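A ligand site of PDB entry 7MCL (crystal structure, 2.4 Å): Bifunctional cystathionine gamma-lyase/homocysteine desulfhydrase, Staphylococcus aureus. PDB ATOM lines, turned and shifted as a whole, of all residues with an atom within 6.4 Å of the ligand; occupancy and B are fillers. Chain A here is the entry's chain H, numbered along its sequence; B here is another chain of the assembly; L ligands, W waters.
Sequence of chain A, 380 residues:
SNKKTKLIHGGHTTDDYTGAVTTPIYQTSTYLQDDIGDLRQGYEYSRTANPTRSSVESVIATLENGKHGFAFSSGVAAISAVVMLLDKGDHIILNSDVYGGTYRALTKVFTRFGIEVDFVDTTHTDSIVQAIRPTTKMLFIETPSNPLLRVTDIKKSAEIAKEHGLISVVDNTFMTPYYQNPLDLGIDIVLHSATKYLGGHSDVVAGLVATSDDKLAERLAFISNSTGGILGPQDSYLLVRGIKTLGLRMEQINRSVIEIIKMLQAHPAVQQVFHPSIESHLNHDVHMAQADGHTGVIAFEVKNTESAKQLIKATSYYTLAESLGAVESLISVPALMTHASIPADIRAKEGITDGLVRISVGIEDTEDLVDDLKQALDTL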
ATOM      1  N   SER A  73     -25.866   8.708   1.426  1.00  0.00           N
ATOM      2  CA  SER A  73     -27.317   8.570   1.357  1.00  0.00           C
ATOM      3  C   SER A  73     -27.826   7.225   1.877  1.00  0.00           C
ATOM      4  O   SER A  73     -29.040   7.016   1.868  1.00  0.00           O
ATOM      5  CB  SER A  73     -27.759   8.784  -0.088  1.00  0.00           C
ATOM      6  OG  SER A  73     -26.931   8.066  -0.973  1.00  0.00           O
ATOM      7  N   SER A  74     -26.952   6.330   2.307  1.00  0.00           N
ATOM      8  CA  SER A  74     -27.346   5.054   2.899  1.00  0.00           C
ATOM      9  C   SER A  74     -26.094   4.408   3.451  1.00  0.00           C
ATOM     10  O   SER A  74     -24.969   4.773   3.066  1.00  0.00           O
ATOM     11  CB  SER A  74     -28.028   4.134   1.902  1.00  0.00           C
ATOM     12  OG  SER A  74     -27.208   3.949   0.766  1.00  0.00           O
ATOM     13  N   GLY A  75     -26.283   3.452   4.346  1.00  0.00           N
ATOM     14  CA  GLY A  75     -25.132   2.673   4.800  1.00  0.00           C
ATOM     15  C   GLY A  75     -24.512   1.868   3.670  1.00  0.00           C
ATOM     16  O   GLY A  75     -23.295   1.650   3.635  1.00  0.00           O
ATOM     17  N   VAL A  76     -25.347   1.403   2.752  1.00  0.00           N
ATOM     18  CA  VAL A  76     -24.853   0.715   1.574  1.00  0.00           C
ATOM     19  C   VAL A  76     -23.992   1.646   0.728  1.00  0.00           C
ATOM     20  O   VAL A  76     -22.950   1.245   0.207  1.00  0.00           O
ATOM     21  CB  VAL A  76     -26.036   0.146   0.778  1.00  0.00           C
ATOM     22  CG1 VAL A  76     -25.618  -0.145  -0.571  1.00  0.00           C
ATOM     23  CG2 VAL A  76     -26.514  -1.138   1.435  1.00  0.00           C
ATOM     24  N   ALA A  77     -24.382   2.919   0.594  1.00  0.00           N
ATOM     25  CA  ALA A  77     -23.548   3.854  -0.146  1.00  0.00           C
ATOM     26  C   ALA A  77     -22.222   4.096   0.564  1.00  0.00           C
ATOM     27  O   ALA A  77     -21.190   4.288  -0.095  1.00  0.00           O
ATOM     28  CB  ALA A  77     -24.300   5.164  -0.383  1.00  0.00           C
ATOM     29  N   ILE A  79     -20.536   1.819   2.581  1.00  0.00           N
ATOM     30  CA  ILE A  79     -19.726   0.635   2.324  1.00  0.00           C
ATOM     31  C   ILE A  79     -19.220   0.648   0.896  1.00  0.00           C
ATOM     32  O   ILE A  79     -18.034   0.423   0.630  1.00  0.00           O
ATOM     33  CB  ILE A  79     -20.560  -0.635   2.590  1.00  0.00           C
ATOM     34  CG1 ILE A  79     -20.849  -0.731   4.086  1.00  0.00           C
ATOM     35  CG2 ILE A  79     -19.859  -1.874   2.033  1.00  0.00           C
ATOM     36  CD1 ILE A  79     -21.996  -1.639   4.391  1.00  0.00           C
ATOM     37  N   VAL A  98     -21.007 -12.314   7.210  1.00  0.00           N
ATOM     38  CA  VAL A  98     -21.552 -11.111   6.602  1.00  0.00           C
ATOM     39  C   VAL A  98     -22.671 -11.507   5.626  1.00  0.00           C
ATOM     40  O   VAL A  98     -22.548 -12.496   4.882  1.00  0.00           O
ATOM     41  CB  VAL A  98     -20.417 -10.335   5.910  1.00  0.00           C
ATOM     42  CG1 VAL A  98     -19.749 -11.194   4.831  1.00  0.00           C
ATOM     43  CG2 VAL A  98     -20.916  -9.028   5.319  1.00  0.00           C
ATOM     44  N   TYR A  99     -23.761 -10.757   5.645  1.00  0.00           N
ATOM     45  CA  TYR A  99     -24.835 -11.005   4.692  1.00  0.00           C
ATOM     46  C   TYR A  99     -25.553  -9.682   4.421  1.00  0.00           C
ATOM     47  O   TYR A  99     -25.027  -8.615   4.744  1.00  0.00           O
ATOM     48  CB  TYR A  99     -25.766 -12.113   5.216  1.00  0.00           C
ATOM     49  CG  TYR A  99     -26.434 -12.910   4.123  1.00  0.00           C
ATOM     50  CD1 TYR A  99     -27.809 -12.884   3.947  1.00  0.00           C
ATOM     51  CD2 TYR A  99     -25.665 -13.691   3.236  1.00  0.00           C
ATOM     52  CE1 TYR A  99     -28.419 -13.629   2.955  1.00  0.00           C
ATOM     53  CE2 TYR A  99     -26.262 -14.427   2.229  1.00  0.00           C
ATOM     54  CZ  TYR A  99     -27.640 -14.385   2.094  1.00  0.00           C
ATOM     55  OH  TYR A  99     -28.272 -15.107   1.104  1.00  0.00           O
ATOM     56  N   GLY A 100     -26.721  -9.758   3.803  1.00  0.00           N
ATOM     57  CA  GLY A 100     -27.486  -8.553   3.533  1.00  0.00           C
ATOM     58  C   GLY A 100     -26.767  -7.604   2.593  1.00  0.00           C
ATOM     59  O   GLY A 100     -26.086  -8.022   1.650  1.00  0.00           O
ATOM     60  N   GLY A 101     -26.893  -6.305   2.885  1.00  0.00           N
ATOM     61  CA  GLY A 101     -26.445  -5.275   1.955  1.00  0.00           C
ATOM     62  C   GLY A 101     -24.971  -5.379   1.590  1.00  0.00           C
ATOM     63  O   GLY A 101     -24.605  -5.284   0.423  1.00  0.00           O
ATOM     64  N   THR A 102     -24.097  -5.539   2.599  1.00  0.00           N
ATOM     65  CA  THR A 102     -22.663  -5.611   2.332  1.00  0.00           C
ATOM     66  C   THR A 102     -22.337  -6.781   1.416  1.00  0.00           C
ATOM     67  O   THR A 102     -21.640  -6.628   0.400  1.00  0.00           O
ATOM     68  CB  THR A 102     -21.891  -5.732   3.645  1.00  0.00           C
ATOM     69  OG1 THR A 102     -22.284  -4.693   4.528  1.00  0.00           O
ATOM     70  CG2 THR A 102     -20.404  -5.597   3.421  1.00  0.00           C
ATOM     71  N   TYR A 103     -22.856  -7.969   1.759  1.00  0.00           N
ATOM     72  CA  TYR A 103     -22.602  -9.150   0.952  1.00  0.00           C
ATOM     73  C   TYR A 103     -23.125  -8.981  -0.462  1.00  0.00           C
ATOM     74  O   TYR A 103     -22.447  -9.314  -1.434  1.00  0.00           O
ATOM     75  CB  TYR A 103     -23.225 -10.376   1.633  1.00  0.00           C
ATOM     76  CG  TYR A 103     -23.101 -11.663   0.845  1.00  0.00           C
ATOM     77  CD1 TYR A 103     -21.936 -12.445   0.930  1.00  0.00           C
ATOM     78  CD2 TYR A 103     -24.149 -12.111   0.037  1.00  0.00           C
ATOM     79  CE1 TYR A 103     -21.826 -13.617   0.211  1.00  0.00           C
ATOM     80  CE2 TYR A 103     -24.039 -13.283  -0.682  1.00  0.00           C
ATOM     81  CZ  TYR A 103     -22.863 -14.033  -0.601  1.00  0.00           C
ATOM     82  OH  TYR A 103     -22.746 -15.203  -1.312  1.00  0.00           O
ATOM     83  N   ARG A 104     -24.351  -8.482  -0.591  1.00  0.00           N
ATOM     84  CA  ARG A 104     -24.939  -8.338  -1.913  1.00  0.00           C
ATOM     85  C   ARG A 104     -24.136  -7.354  -2.759  1.00  0.00           C
ATOM     86  O   ARG A 104     -23.809  -7.643  -3.915  1.00  0.00           O
ATOM     87  CB  ARG A 104     -26.400  -7.907  -1.784  1.00  0.00           C
ATOM     88  CG  ARG A 104     -27.151  -7.724  -3.104  1.00  0.00           C
ATOM     89  CD  ARG A 104     -28.568  -7.158  -2.853  1.00  0.00           C
ATOM     90  NE  ARG A 104     -29.002  -7.316  -1.458  1.00  0.00           N
ATOM     91  CZ  ARG A 104     -29.635  -8.392  -0.967  1.00  0.00           C
ATOM     92  NH1 ARG A 104     -29.967  -8.425   0.320  1.00  0.00           N
ATOM     93  NH2 ARG A 104     -29.919  -9.425  -1.753  1.00  0.00           N
ATOM     94  N   GLU A 142     -17.341  -6.781  10.722  1.00  0.00           N
ATOM     95  CA  GLU A 142     -18.506  -6.411  11.500  1.00  0.00           C
ATOM     96  C   GLU A 142     -18.392  -7.064  12.862  1.00  0.00           C
ATOM     97  O   GLU A 142     -18.149  -8.282  12.954  1.00  0.00           O
ATOM     98  CB  GLU A 142     -19.791  -6.910  10.837  1.00  0.00           C
ATOM     99  CG  GLU A 142     -19.982  -6.579   9.398  1.00  0.00           C
ATOM    100  CD  GLU A 142     -21.186  -7.324   8.868  1.00  0.00           C
ATOM    101  OE1 GLU A 142     -21.331  -8.512   9.240  1.00  0.00           O
ATOM    102  OE2 GLU A 142     -22.004  -6.724   8.122  1.00  0.00           O
ATOM    103  N   ASN A 146     -24.287 -10.176  12.403  1.00  0.00           N
ATOM    104  CA  ASN A 146     -25.707 -10.458  12.351  1.00  0.00           C
ATOM    105  C   ASN A 146     -25.947 -11.830  11.724  1.00  0.00           C
ATOM    106  O   ASN A 146     -25.245 -12.207  10.780  1.00  0.00           O
ATOM    107  CB  ASN A 146     -26.415  -9.376  11.520  1.00  0.00           C
ATOM    108  CG  ASN A 146     -27.896  -9.601  11.414  1.00  0.00           C
ATOM    109  OD1 ASN A 146     -28.619  -9.537  12.392  1.00  0.00           O
ATOM    110  ND2 ASN A 146     -28.366  -9.890  10.219  1.00  0.00           N
ATOM    111  N   ASP A 171     -17.406  -2.094  10.597  1.00  0.00           N
ATOM    112  CA  ASP A 171     -18.822  -1.752  10.622  1.00  0.00           C
ATOM    113  C   ASP A 171     -19.251  -1.741  12.084  1.00  0.00           C
ATOM    114  O   ASP A 171     -19.437  -2.792  12.697  1.00  0.00           O
ATOM    115  CB  ASP A 171     -19.645  -2.731   9.808  1.00  0.00           C
ATOM    116  CG  ASP A 171     -21.104  -2.302   9.660  1.00  0.00           C
ATOM    117  OD1 ASP A 171     -21.605  -1.595  10.566  1.00  0.00           O
ATOM    118  OD2 ASP A 171     -21.744  -2.671   8.653  1.00  0.00           O
ATOM    119  N   HIS A 192     -20.962   3.205   9.644  1.00  0.00           N
ATOM    120  CA  HIS A 192     -22.265   2.983  10.241  1.00  0.00           C
ATOM    121  C   HIS A 192     -23.344   3.062   9.178  1.00  0.00           C
ATOM    122  O   HIS A 192     -23.276   3.891   8.256  1.00  0.00           O
ATOM    123  CB  HIS A 192     -22.619   4.036  11.292  1.00  0.00           C
ATOM    124  CG  HIS A 192     -21.690   4.066  12.455  1.00  0.00           C
ATOM    125  ND1 HIS A 192     -21.968   3.442  13.660  1.00  0.00           N
ATOM    126  CD2 HIS A 192     -20.475   4.663  12.609  1.00  0.00           C
ATOM    127  CE1 HIS A 192     -20.967   3.649  14.497  1.00  0.00           C
ATOM    128  NE2 HIS A 192     -20.044   4.384  13.886  1.00  0.00           N
ATOM    129  N   SER A 193     -24.351   2.208   9.329  1.00  0.00           N
ATOM    130  CA  SER A 193     -25.675   2.486   8.789  1.00  0.00           C
ATOM    131  C   SER A 193     -26.374   3.380   9.820  1.00  0.00           C
ATOM    132  O   SER A 193     -26.971   2.905  10.790  1.00  0.00           O
ATOM    133  CB  SER A 193     -26.449   1.196   8.536  1.00  0.00           C
ATOM    134  OG  SER A 193     -27.763   1.487   8.122  1.00  0.00           O
ATOM    135  N   ALA A 194     -26.276   4.686   9.616  1.00  0.00           N
ATOM    136  CA  ALA A 194     -26.879   5.640  10.532  1.00  0.00           C
ATOM    137  C   ALA A 194     -28.411   5.525  10.559  1.00  0.00           C
ATOM    138  O   ALA A 194     -29.049   6.101  11.441  1.00  0.00           O
ATOM    139  CB  ALA A 194     -26.449   7.053  10.138  1.00  0.00           C
ATOM    140  N   THR A 195     -28.987   4.795   9.615  1.00  0.00           N
ATOM    141  CA  THR A 195     -30.415   4.477   9.620  1.00  0.00           C
ATOM    142  C   THR A 195     -30.871   3.834  10.924  1.00  0.00           C
ATOM    143  O   THR A 195     -32.059   3.887  11.258  1.00  0.00           O
ATOM    144  CB  THR A 195     -30.684   3.529   8.443  1.00  0.00           C
ATOM    145  OG1 THR A 195     -30.138   4.093   7.239  1.00  0.00           O
ATOM    146  CG2 THR A 195     -32.141   3.277   8.253  1.00  0.00           C
ATOM    147  N   LYS A 196     -29.943   3.228  11.680  1.00  0.00           N
ATOM    148  CA  LYS A 196     -30.281   2.372  12.800  1.00  0.00           C
ATOM    149  C   LYS A 196     -30.268   3.184  14.077  1.00  0.00           C
ATOM    150  O   LYS A 196     -31.117   4.061  14.246  1.00  0.00           O
ATOM    151  CB  LYS A 196     -29.303   1.214  12.919  1.00  0.00           C
ATOM    152  CG  LYS A 196     -29.120   0.449  11.618  1.00  0.00           C
ATOM    153  CD  LYS A 196     -30.384  -0.253  11.229  1.00  0.00           C
ATOM    154  CE  LYS A 196     -30.163  -1.229  10.063  1.00  0.00           C
ATOM    155  NZ  LYS A 196     -29.967  -0.546   8.754  1.00  0.00           N
ATOM    156  N   VAL A 204     -34.693   8.189   8.899  1.00  0.00           N
ATOM    157  CA  VAL A 204     -33.573   8.669   8.096  1.00  0.00           C
ATOM    158  C   VAL A 204     -32.841   7.472   7.528  1.00  0.00           C
ATOM    159  O   VAL A 204     -32.504   6.541   8.267  1.00  0.00           O
ATOM    160  CB  VAL A 204     -32.587   9.536   8.895  1.00  0.00           C
ATOM    161  CG1 VAL A 204     -31.452   9.966   8.006  1.00  0.00           C
ATOM    162  CG2 VAL A 204     -33.269  10.751   9.468  1.00  0.00           C
ATOM    163  N   VAL A 205     -32.569   7.499   6.229  1.00  0.00           N
ATOM    164  CA  VAL A 205     -31.719   6.520   5.587  1.00  0.00           C
ATOM    165  C   VAL A 205     -30.374   7.188   5.332  1.00  0.00           C
ATOM    166  O   VAL A 205     -30.302   8.198   4.613  1.00  0.00           O
ATOM    167  CB  VAL A 205     -32.353   5.997   4.291  1.00  0.00           C
ATOM    168  CG1 VAL A 205     -31.462   5.017   3.599  1.00  0.00           C
ATOM    169  CG2 VAL A 205     -33.710   5.358   4.620  1.00  0.00           C
ATOM    170  N   ALA A 206     -29.322   6.669   5.956  1.00  0.00           N
ATOM    171  CA  ALA A 206     -28.051   7.387   5.922  1.00  0.00           C
ATOM    172  C   ALA A 206     -26.921   6.434   6.269  1.00  0.00           C
ATOM    173  O   ALA A 206     -27.116   5.450   6.999  1.00  0.00           O
ATOM    174  CB  ALA A 206     -28.057   8.575   6.898  1.00  0.00           C
ATOM    175  N   GLY A 207     -25.733   6.750   5.756  1.00  0.00           N
ATOM    176  CA  GLY A 207     -24.508   6.057   6.136  1.00  0.00           C
ATOM    177  C   GLY A 207     -23.498   7.078   6.618  1.00  0.00           C
ATOM    178  O   GLY A 207     -23.490   8.220   6.176  1.00  0.00           O
ATOM    179  N   THR A 338     -34.407 -12.606   6.327  1.00  0.00           N
ATOM    180  CA  THR A 338     -33.112 -12.226   5.771  1.00  0.00           C
ATOM    181  C   THR A 338     -32.421 -13.386   5.054  1.00  0.00           C
ATOM    182  O   THR A 338     -31.695 -13.167   4.079  1.00  0.00           O
ATOM    183  CB  THR A 338     -32.209 -11.676   6.869  1.00  0.00           C
ATOM    184  OG1 THR A 338     -32.182 -12.587   7.969  1.00  0.00           O
ATOM    185  CG2 THR A 338     -32.712 -10.327   7.344  1.00  0.00           C
ATOM    186  N   ARG B  47     -34.190  -1.358  -1.285  1.00  0.00           N
ATOM    187  CA  ARG B  47     -34.983  -0.350  -0.578  1.00  0.00           C
ATOM    188  C   ARG B  47     -36.439  -0.667  -0.809  1.00  0.00           C
ATOM    189  O   ARG B  47     -36.823  -1.059  -1.922  1.00  0.00           O
ATOM    190  CB  ARG B  47     -34.652   1.076  -1.063  1.00  0.00           C
ATOM    191  CG  ARG B  47     -33.170   1.427  -1.056  1.00  0.00           C
ATOM    192  CD  ARG B  47     -32.617   1.849   0.322  1.00  0.00           C
ATOM    193  NE  ARG B  47     -31.225   1.431   0.557  1.00  0.00           N
ATOM    194  CZ  ARG B  47     -30.466   0.764  -0.319  1.00  0.00           C
ATOM    195  N   GLY B 228     -26.907   2.169  -3.290  1.00  0.00           N
ATOM    196  CA  GLY B 228     -27.533   3.026  -2.303  1.00  0.00           C
ATOM    197  C   GLY B 228     -27.465   4.528  -2.523  1.00  0.00           C
ATOM    198  O   GLY B 228     -27.629   5.286  -1.554  1.00  0.00           O
HETATM  199  N1  LIG L   1     -25.875  -2.848   5.700  1.00  0.00           N
HETATM  200  C1  LIG L   1     -24.981  -5.137   5.834  1.00  0.00           C
HETATM  201  C2  LIG L   1     -27.420  -4.659   5.473  1.00  0.00           C
HETATM  202  O1  LIG L   1     -27.674  -5.992   5.427  1.00  0.00           O
HETATM  203  C3  LIG L   1     -29.838  -4.342   5.116  1.00  0.00           C
HETATM  204  O2  LIG L   1     -30.077  -5.501   4.797  1.00  0.00           O
HETATM  205  C4  LIG L   1     -28.226  -2.409   5.363  1.00  0.00           C
HETATM  206  C5  LIG L   1     -26.906  -1.990   5.573  1.00  0.00           C
HETATM  207  C6  LIG L   1     -29.322  -1.391   5.218  1.00  0.00           C
HETATM  208  O3  LIG L   1     -28.842  -0.155   5.711  1.00  0.00           O
HETATM  209  P1  LIG L   1     -29.212   1.156   4.863  1.00  0.00           P
HETATM  210  O4  LIG L   1     -28.611   1.024   3.476  1.00  0.00           O
HETATM  211  O5  LIG L   1     -30.711   1.196   4.797  1.00  0.00           O
HETATM  212  O6  LIG L   1     -28.668   2.349   5.610  1.00  0.00           O
HETATM  213  O   HOH W   1     -30.790  -6.415   2.232  1.00  0.00           O
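N of Gly 101 is in hydrogen-bond range of O1 of the ligand, at 2.7 Å.
O6 of the ligand lies within hydrogen-bond range of OG1 of Thr 195, at 2.8 Å.
An oxygen (O6) of the ligand is in hydrogen-bond range of the side-chain hydroxyl of Ser 193.
The backbone NH (N) of Gly 75 lies within hydrogen-bond range of an oxygen (O6) of the ligand (2.9 Å).
An oxygen (O3) of the ligand lies within hydrogen-bond range of the side-chain amino group (NZ) of Lys 196, 3.3 Å away.
The backbone NH of Val 76 is in hydrogen-bond range of an oxygen (O4) of the ligand, 3.4 Å away.
O4 of the ligand lies within salt-bridge range of NE of Arg 47 of chain B, at 3.9 Å.
N of Ala 206 lies within hydrogen-bond range of OG1 of Thr 195.
The side-chain hydroxyl (OG) of Ser 193 is in hydrogen-bond range of the side-chain amino group (NZ) of Lys 196, 3.1 Å away.
N of Gly 75 is in hydrogen-bond range of O of Ala 206, at 3.4 Å.
O of Ser 74 sits close to N of Gly 207, at 3.4 Å.
OG of Ser 74 is in hydrogen-bond range of N of Ala 77, at 3.0 Å.
O of Gly 228 of chain B is in hydrogen-bond range of OG of Ser 74, 2.7 Å away.
The backbone NH (N) of Ala 194 is in hydrogen-bond range of the backbone carbonyl oxygen (O) of Ala 206 (2.9 Å).
Ser 74 touches the ligand.
Tyr 99 touches the ligand (O to C1, 3.6 Å).
Gly 100 touches the ligand (CA to O1, 3.2 Å).
Thr 102 touches the ligand (OG1 to C1, 3.0 Å).
O of Ala 206 touches O6 of the ligand, at 3.7 Å.
Along chain A the residues within 4 Å of the ligand span positions 74 to 206.
Water W1 lies within hydrogen-bond range of an oxygen (O2) of the ligand and the guanidinium group (NH1) of Arg 104.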
